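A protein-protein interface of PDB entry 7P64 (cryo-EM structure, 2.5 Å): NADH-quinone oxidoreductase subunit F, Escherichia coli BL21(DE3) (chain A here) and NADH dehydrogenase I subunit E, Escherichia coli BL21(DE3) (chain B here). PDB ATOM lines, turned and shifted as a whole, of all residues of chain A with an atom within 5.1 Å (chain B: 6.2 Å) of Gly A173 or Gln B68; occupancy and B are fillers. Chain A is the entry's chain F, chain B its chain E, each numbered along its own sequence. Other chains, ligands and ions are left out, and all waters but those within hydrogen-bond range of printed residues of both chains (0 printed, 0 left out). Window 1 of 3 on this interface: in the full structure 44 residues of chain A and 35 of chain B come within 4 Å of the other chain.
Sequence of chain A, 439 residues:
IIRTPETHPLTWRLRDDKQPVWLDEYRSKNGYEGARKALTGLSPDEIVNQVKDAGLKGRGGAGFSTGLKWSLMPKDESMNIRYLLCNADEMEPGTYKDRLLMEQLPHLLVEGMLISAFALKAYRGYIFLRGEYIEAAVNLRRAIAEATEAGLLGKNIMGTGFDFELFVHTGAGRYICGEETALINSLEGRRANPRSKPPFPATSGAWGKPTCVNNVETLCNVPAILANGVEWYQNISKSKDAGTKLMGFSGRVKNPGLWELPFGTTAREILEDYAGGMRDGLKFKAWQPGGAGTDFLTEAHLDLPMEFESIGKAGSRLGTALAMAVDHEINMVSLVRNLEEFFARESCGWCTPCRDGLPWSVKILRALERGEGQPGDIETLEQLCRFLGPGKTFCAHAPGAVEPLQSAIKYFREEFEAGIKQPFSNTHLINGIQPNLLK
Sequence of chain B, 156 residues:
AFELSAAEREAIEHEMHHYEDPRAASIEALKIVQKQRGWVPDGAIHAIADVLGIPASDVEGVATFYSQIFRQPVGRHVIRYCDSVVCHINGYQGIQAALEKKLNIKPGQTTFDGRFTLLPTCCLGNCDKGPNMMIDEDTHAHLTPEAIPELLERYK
The side-chain sulfur of Cys B122 lies within hydrogen-bond range of the side-chain sulfur of Met A91.
The side-chain carboxylate (OE2) of Glu A132 lies within salt-bridge range of the guanidinium group (NH2) of Arg B80 (2.9 Å).
The backbone carbonyl oxygen (O) of Gly A171 is in hydrogen-bond range of the side-chain amino group (NZ) of Lys B31 (3.0 Å).
The backbone carbonyl oxygen (O) of Ala A172 lies close to the backbone NH (N) of Gln B68 (3.3 Å).
The backbone carbonyl oxygen (O) of Gly A173 is in hydrogen-bond range of the side-chain hydroxyl (OG) of Ser B67 (2.8 Å).
The guanidinium group (NH2) of Arg A174 sits at hydrogen-bond distance from the backbone carbonyl oxygen (O) of Phe B65 (2.5 Å).
NH1 of Arg A174 is in salt-bridge range of OE1 of Glu A346, 3.7 Å away.
The backbone carbonyl oxygen of Gln B68 is in hydrogen-bond range of the side-chain amide nitrogen of Gln B34, at 2.4 Å.
NE2 of Gln B68 lies within hydrogen-bond range of OG of Ser B67.
OE1 of Gln B68 lies within hydrogen-bond range of NE of Arg B80, 3.0 Å away.
The side-chain hydroxyl of Thr B121 sits at hydrogen-bond distance from the guanidinium group of Arg B80, 2.9 Å away.
Among the printed residues, merely in contact across the chains: Glu A132 with Gln B68 (3.6 Å), Ala A172 with Tyr B66 (3.3 Å), Ala A172 with Ser B67 (3.8 Å), Ala A172 with Ile B69 (3.9 Å), Gly A173 with Gln B68 (3.8 Å), Arg A174 with Tyr B66 (3.8 Å) and Arg A174 with Ser B67 (3.6 Å).
Gly A173 touches just these residues of chain B: Ser B67 (2.8 Å) and Gln B68 (3.8 Å).
Of the printed residues of chain A, Tyr B66 touches Ala A172 (3.3 Å) and Arg A174 (3.8 Å).
Gln B68 touches just these residues of chain A: Glu A132, Ala A172 and Gly A173.
Of the printed residues of chain A, Ile B69 touches Ala A172 (3.9 Å).
Of the printed residues of chain A, Cys B122 touches Met A91.
The nearest printed residue of chain A that does not touch Gln B68 is Gly A171 (5.8 Å).
The nearest printed residue of chain A that does not touch Phe B65 is Gly A173 (5.5 Å).
Along chain B the printed residues that touch a printed residue of chain A span positions 31 to 122.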
ATOM      1  N   MET A  91      -7.686 -25.589  15.262  1.00  0.00           N
ATOM      2  CA  MET A  91      -6.895 -24.977  14.208  1.00  0.00           C
ATOM      3  C   MET A  91      -6.708 -23.479  14.394  1.00  0.00           C
ATOM      4  O   MET A  91      -6.060 -22.843  13.556  1.00  0.00           O
ATOM      5  CB  MET A  91      -7.536 -25.259  12.848  1.00  0.00           C
ATOM      6  CG  MET A  91      -6.947 -26.461  12.145  1.00  0.00           C
ATOM      7  SD  MET A  91      -5.717 -26.009  10.920  1.00  0.00           S
ATOM      8  CE  MET A  91      -5.362 -27.609  10.212  1.00  0.00           C
ATOM      9  N   GLU A 132      -2.216 -32.873  12.033  1.00  0.00           N
ATOM     10  CA  GLU A 132      -0.903 -32.514  12.546  1.00  0.00           C
ATOM     11  C   GLU A 132      -0.640 -33.079  13.933  1.00  0.00           C
ATOM     12  O   GLU A 132       0.513 -33.080  14.375  1.00  0.00           O
ATOM     13  CB  GLU A 132      -0.749 -30.992  12.573  1.00  0.00           C
ATOM     14  CG  GLU A 132      -0.517 -30.362  11.210  1.00  0.00           C
ATOM     15  CD  GLU A 132      -1.788 -30.244  10.390  1.00  0.00           C
ATOM     16  OE1 GLU A 132      -2.817 -29.803  10.942  1.00  0.00           O
ATOM     17  OE2 GLU A 132      -1.758 -30.599   9.194  1.00  0.00           O
ATOM     18  N   GLY A 171      -8.018 -35.255  10.221  1.00  0.00           N
ATOM     19  CA  GLY A 171      -8.302 -34.256   9.217  1.00  0.00           C
ATOM     20  C   GLY A 171      -7.207 -34.148   8.174  1.00  0.00           C
ATOM     21  O   GLY A 171      -6.181 -34.825   8.221  1.00  0.00           O
ATOM     22  N   ALA A 172      -7.440 -33.265   7.209  1.00  0.00           N
ATOM     23  CA  ALA A 172      -6.520 -33.059   6.100  1.00  0.00           C
ATOM     24  C   ALA A 172      -6.161 -31.589   5.956  1.00  0.00           C
ATOM     25  O   ALA A 172      -5.973 -31.083   4.847  1.00  0.00           O
ATOM     26  CB  ALA A 172      -7.101 -33.603   4.799  1.00  0.00           C
ATOM     27  N   GLY A 173      -6.069 -30.878   7.073  1.00  0.00           N
ATOM     28  CA  GLY A 173      -5.488 -29.551   7.065  1.00  0.00           C
ATOM     29  C   GLY A 173      -6.333 -28.434   6.490  1.00  0.00           C
ATOM     30  O   GLY A 173      -6.016 -27.905   5.422  1.00  0.00           O
ATOM     31  N   ARG A 174      -7.415 -28.069   7.173  1.00  0.00           N
ATOM     32  CA  ARG A 174      -8.180 -26.888   6.799  1.00  0.00           C
ATOM     33  C   ARG A 174      -8.772 -26.274   8.059  1.00  0.00           C
ATOM     34  O   ARG A 174      -9.326 -26.991   8.896  1.00  0.00           O
ATOM     35  CB  ARG A 174      -9.276 -27.238   5.786  1.00  0.00           C
ATOM     36  CG  ARG A 174      -9.868 -26.045   5.065  1.00  0.00           C
ATOM     37  CD  ARG A 174      -8.799 -25.167   4.439  1.00  0.00           C
ATOM     38  NE  ARG A 174      -8.366 -25.627   3.126  1.00  0.00           N
ATOM     39  CZ  ARG A 174      -7.460 -25.007   2.381  1.00  0.00           C
ATOM     40  NH1 ARG A 174      -6.862 -23.904   2.798  1.00  0.00           N
ATOM     41  NH2 ARG A 174      -7.150 -25.503   1.189  1.00  0.00           N
ATOM     42  N   TYR A 175      -8.644 -24.951   8.190  1.00  0.00           N
ATOM     43  CA  TYR A 175      -9.051 -24.272   9.416  1.00  0.00           C
ATOM     44  C   TYR A 175     -10.565 -24.244   9.583  1.00  0.00           C
ATOM     45  O   TYR A 175     -11.061 -24.333  10.711  1.00  0.00           O
ATOM     46  CB  TYR A 175      -8.491 -22.850   9.433  1.00  0.00           C
ATOM     47  CG  TYR A 175      -9.135 -21.927  10.444  1.00  0.00           C
ATOM     48  CD1 TYR A 175      -8.843 -22.035  11.795  1.00  0.00           C
ATOM     49  CD2 TYR A 175     -10.025 -20.941  10.045  1.00  0.00           C
ATOM     50  CE1 TYR A 175      -9.422 -21.193  12.718  1.00  0.00           C
ATOM     51  CE2 TYR A 175     -10.607 -20.097  10.962  1.00  0.00           C
ATOM     52  CZ  TYR A 175     -10.302 -20.226  12.295  1.00  0.00           C
ATOM     53  OH  TYR A 175     -10.885 -19.383  13.210  1.00  0.00           O
ATOM     54  N   GLU A 346      -7.710 -19.184   4.557  1.00  0.00           N
ATOM     55  CA  GLU A 346      -8.482 -20.257   5.170  1.00  0.00           C
ATOM     56  C   GLU A 346      -9.977 -20.072   4.978  1.00  0.00           C
ATOM     57  O   GLU A 346     -10.768 -20.755   5.635  1.00  0.00           O
ATOM     58  CB  GLU A 346      -8.147 -20.376   6.655  1.00  0.00           C
ATOM     59  CG  GLU A 346      -6.724 -20.821   6.916  1.00  0.00           C
ATOM     60  CD  GLU A 346      -6.386 -22.147   6.273  1.00  0.00           C
ATOM     61  OE1 GLU A 346      -7.211 -23.076   6.353  1.00  0.00           O
ATOM     62  OE2 GLU A 346      -5.290 -22.261   5.691  1.00  0.00           O
ATOM     63  N   LYS B  31      -5.751 -39.703   1.703  1.00  0.00           N
ATOM     64  CA  LYS B  31      -4.582 -39.716   2.577  1.00  0.00           C
ATOM     65  C   LYS B  31      -3.831 -41.041   2.504  1.00  0.00           C
ATOM     66  O   LYS B  31      -2.607 -41.054   2.632  1.00  0.00           O
ATOM     67  CB  LYS B  31      -4.994 -39.414   4.015  1.00  0.00           C
ATOM     68  CG  LYS B  31      -4.888 -37.946   4.380  1.00  0.00           C
ATOM     69  CD  LYS B  31      -5.867 -37.567   5.474  1.00  0.00           C
ATOM     70  CE  LYS B  31      -5.616 -38.364   6.739  1.00  0.00           C
ATOM     71  NZ  LYS B  31      -4.903 -37.555   7.762  1.00  0.00           N
ATOM     72  N   GLN B  34      -1.893 -40.838  -0.704  1.00  0.00           N
ATOM     73  CA  GLN B  34      -0.805 -39.891  -0.488  1.00  0.00           C
ATOM     74  C   GLN B  34       0.307 -40.494   0.365  1.00  0.00           C
ATOM     75  O   GLN B  34       1.490 -40.277   0.092  1.00  0.00           O
ATOM     76  CB  GLN B  34      -1.350 -38.620   0.159  1.00  0.00           C
ATOM     77  CG  GLN B  34      -0.293 -37.611   0.547  1.00  0.00           C
ATOM     78  CD  GLN B  34      -0.824 -36.201   0.568  1.00  0.00           C
ATOM     79  OE1 GLN B  34      -1.241 -35.670  -0.458  1.00  0.00           O
ATOM     80  NE2 GLN B  34      -0.817 -35.584   1.741  1.00  0.00           N
ATOM     81  N   PHE B  65      -9.775 -29.167  -2.123  1.00  0.00           N
ATOM     82  CA  PHE B  65     -10.184 -28.329  -1.001  1.00  0.00           C
ATOM     83  C   PHE B  65      -9.147 -28.348   0.114  1.00  0.00           C
ATOM     84  O   PHE B  65      -8.807 -27.298   0.668  1.00  0.00           O
ATOM     85  CB  PHE B  65     -11.542 -28.780  -0.470  1.00  0.00           C
ATOM     86  CG  PHE B  65     -12.110 -27.870   0.575  1.00  0.00           C
ATOM     87  CD1 PHE B  65     -12.783 -26.719   0.214  1.00  0.00           C
ATOM     88  CD2 PHE B  65     -11.966 -28.159   1.920  1.00  0.00           C
ATOM     89  CE1 PHE B  65     -13.306 -25.878   1.169  1.00  0.00           C
ATOM     90  CE2 PHE B  65     -12.481 -27.319   2.878  1.00  0.00           C
ATOM     91  CZ  PHE B  65     -13.153 -26.179   2.502  1.00  0.00           C
ATOM     92  N   TYR B  66      -8.634 -29.524   0.458  1.00  0.00           N
ATOM     93  CA  TYR B  66      -7.772 -29.677   1.621  1.00  0.00           C
ATOM     94  C   TYR B  66      -6.315 -29.496   1.224  1.00  0.00           C
ATOM     95  O   TYR B  66      -5.840 -30.118   0.270  1.00  0.00           O
ATOM     96  CB  TYR B  66      -7.994 -31.040   2.273  1.00  0.00           C
ATOM     97  CG  TYR B  66      -9.379 -31.184   2.844  1.00  0.00           C
ATOM     98  CD1 TYR B  66      -9.718 -30.591   4.048  1.00  0.00           C
ATOM     99  CD2 TYR B  66     -10.357 -31.889   2.166  1.00  0.00           C
ATOM    100  CE1 TYR B  66     -10.986 -30.711   4.563  1.00  0.00           C
ATOM    101  CE2 TYR B  66     -11.627 -32.010   2.670  1.00  0.00           C
ATOM    102  CZ  TYR B  66     -11.937 -31.421   3.870  1.00  0.00           C
ATOM    103  OH  TYR B  66     -13.205 -31.542   4.379  1.00  0.00           O
ATOM    104  N   SER B  67      -5.611 -28.639   1.965  1.00  0.00           N
ATOM    105  CA  SER B  67      -4.247 -28.272   1.610  1.00  0.00           C
ATOM    106  C   SER B  67      -3.246 -29.387   1.872  1.00  0.00           C
ATOM    107  O   SER B  67      -2.188 -29.408   1.236  1.00  0.00           O
ATOM    108  CB  SER B  67      -3.834 -27.014   2.372  1.00  0.00           C
ATOM    109  OG  SER B  67      -3.899 -27.225   3.771  1.00  0.00           O
ATOM    110  N   GLN B  68      -3.547 -30.310   2.781  1.00  0.00           N
ATOM    111  CA  GLN B  68      -2.622 -31.386   3.110  1.00  0.00           C
ATOM    112  C   GLN B  68      -2.754 -32.588   2.187  1.00  0.00           C
ATOM    113  O   GLN B  68      -2.043 -33.578   2.381  1.00  0.00           O
ATOM    114  CB  GLN B  68      -2.813 -31.824   4.565  1.00  0.00           C
ATOM    115  CG  GLN B  68      -2.247 -30.875   5.634  1.00  0.00           C
ATOM    116  CD  GLN B  68      -1.262 -29.832   5.110  1.00  0.00           C
ATOM    117  OE1 GLN B  68      -0.160 -30.156   4.660  1.00  0.00           O
ATOM    118  NE2 GLN B  68      -1.665 -28.569   5.167  1.00  0.00           N
ATOM    119  N   ILE B  69      -3.641 -32.531   1.203  1.00  0.00           N
ATOM    120  CA  ILE B  69      -3.713 -33.530   0.146  1.00  0.00           C
ATOM    121  C   ILE B  69      -3.063 -32.916  -1.085  1.00  0.00           C
ATOM    122  O   ILE B  69      -3.557 -31.924  -1.630  1.00  0.00           O
ATOM    123  CB  ILE B  69      -5.156 -33.964  -0.132  1.00  0.00           C
ATOM    124  CG1 ILE B  69      -5.718 -34.717   1.071  1.00  0.00           C
ATOM    125  CG2 ILE B  69      -5.221 -34.823  -1.380  1.00  0.00           C
ATOM    126  CD1 ILE B  69      -7.216 -34.826   1.070  1.00  0.00           C
ATOM    127  N   PHE B  70      -1.950 -33.495  -1.521  1.00  0.00           N
ATOM    128  CA  PHE B  70      -1.146 -32.920  -2.589  1.00  0.00           C
ATOM    129  C   PHE B  70      -1.596 -33.480  -3.930  1.00  0.00           C
ATOM    130  O   PHE B  70      -1.551 -34.693  -4.149  1.00  0.00           O
ATOM    131  CB  PHE B  70       0.336 -33.200  -2.359  1.00  0.00           C
ATOM    132  CG  PHE B  70       0.846 -32.695  -1.046  1.00  0.00           C
ATOM    133  CD1 PHE B  70       0.497 -31.436  -0.593  1.00  0.00           C
ATOM    134  CD2 PHE B  70       1.672 -33.477  -0.263  1.00  0.00           C
ATOM    135  CE1 PHE B  70       0.963 -30.968   0.616  1.00  0.00           C
ATOM    136  CE2 PHE B  70       2.141 -33.015   0.947  1.00  0.00           C
ATOM    137  CZ  PHE B  70       1.786 -31.759   1.387  1.00  0.00           C
ATOM    138  N   ARG B  80       7.038 -28.109   6.415  1.00  0.00           N
ATOM    139  CA  ARG B  80       5.878 -27.239   6.581  1.00  0.00           C
ATOM    140  C   ARG B  80       6.159 -26.329   7.771  1.00  0.00           C
ATOM    141  O   ARG B  80       6.076 -26.757   8.925  1.00  0.00           O
ATOM    142  CB  ARG B  80       4.598 -28.043   6.771  1.00  0.00           C
ATOM    143  CG  ARG B  80       4.181 -28.791   5.519  1.00  0.00           C
ATOM    144  CD  ARG B  80       3.059 -29.764   5.787  1.00  0.00           C
ATOM    145  NE  ARG B  80       1.988 -29.148   6.559  1.00  0.00           N
ATOM    146  CZ  ARG B  80       1.451 -29.673   7.651  1.00  0.00           C
ATOM    147  NH1 ARG B  80       1.866 -30.830   8.136  1.00  0.00           N
ATOM    148  NH2 ARG B  80       0.471 -29.022   8.268  1.00  0.00           N
ATOM    149  N   LEU B 119       6.997 -25.496   2.267  1.00  0.00           N
ATOM    150  CA  LEU B 119       5.616 -25.065   2.283  1.00  0.00           C
ATOM    151  C   LEU B 119       5.324 -24.290   3.562  1.00  0.00           C
ATOM    152  O   LEU B 119       5.715 -24.732   4.660  1.00  0.00           O
ATOM    153  CB  LEU B 119       4.670 -26.264   2.173  1.00  0.00           C
ATOM    154  CG  LEU B 119       4.401 -26.838   0.782  1.00  0.00           C
ATOM    155  CD1 LEU B 119       3.655 -28.152   0.890  1.00  0.00           C
ATOM    156  CD2 LEU B 119       3.624 -25.847  -0.061  1.00  0.00           C
ATOM    157  N   PRO B 120       4.665 -23.141   3.464  1.00  0.00           N
ATOM    158  CA  PRO B 120       4.061 -22.544   4.654  1.00  0.00           C
ATOM    159  C   PRO B 120       2.836 -23.339   5.065  1.00  0.00           C
ATOM    160  O   PRO B 120       2.207 -24.024   4.254  1.00  0.00           O
ATOM    161  CB  PRO B 120       3.686 -21.134   4.192  1.00  0.00           C
ATOM    162  CG  PRO B 120       3.452 -21.282   2.738  1.00  0.00           C
ATOM    163  CD  PRO B 120       4.399 -22.347   2.253  1.00  0.00           C
ATOM    164  N   THR B 121       2.501 -23.251   6.344  1.00  0.00           N
ATOM    165  CA  THR B 121       1.360 -23.983   6.861  1.00  0.00           C
ATOM    166  C   THR B 121       0.722 -23.167   7.970  1.00  0.00           C
ATOM    167  O   THR B 121       1.325 -22.238   8.508  1.00  0.00           O
ATOM    168  CB  THR B 121       1.759 -25.381   7.358  1.00  0.00           C
ATOM    169  OG1 THR B 121       0.598 -26.214   7.436  1.00  0.00           O
ATOM    170  CG2 THR B 121       2.427 -25.313   8.720  1.00  0.00           C
ATOM    171  N   CYS B 122      -0.501 -23.539   8.318  1.00  0.00           N
ATOM    172  CA  CYS B 122      -1.250 -22.848   9.357  1.00  0.00           C
ATOM    173  C   CYS B 122      -0.643 -23.170  10.723  1.00  0.00           C
ATOM    174  O   CYS B 122       0.393 -23.829  10.840  1.00  0.00           O
ATOM    175  CB  CYS B 122      -2.723 -23.228   9.275  1.00  0.00           C
ATOM    176  SG  CYS B 122      -3.004 -24.957   8.858  1.00  0.00           S
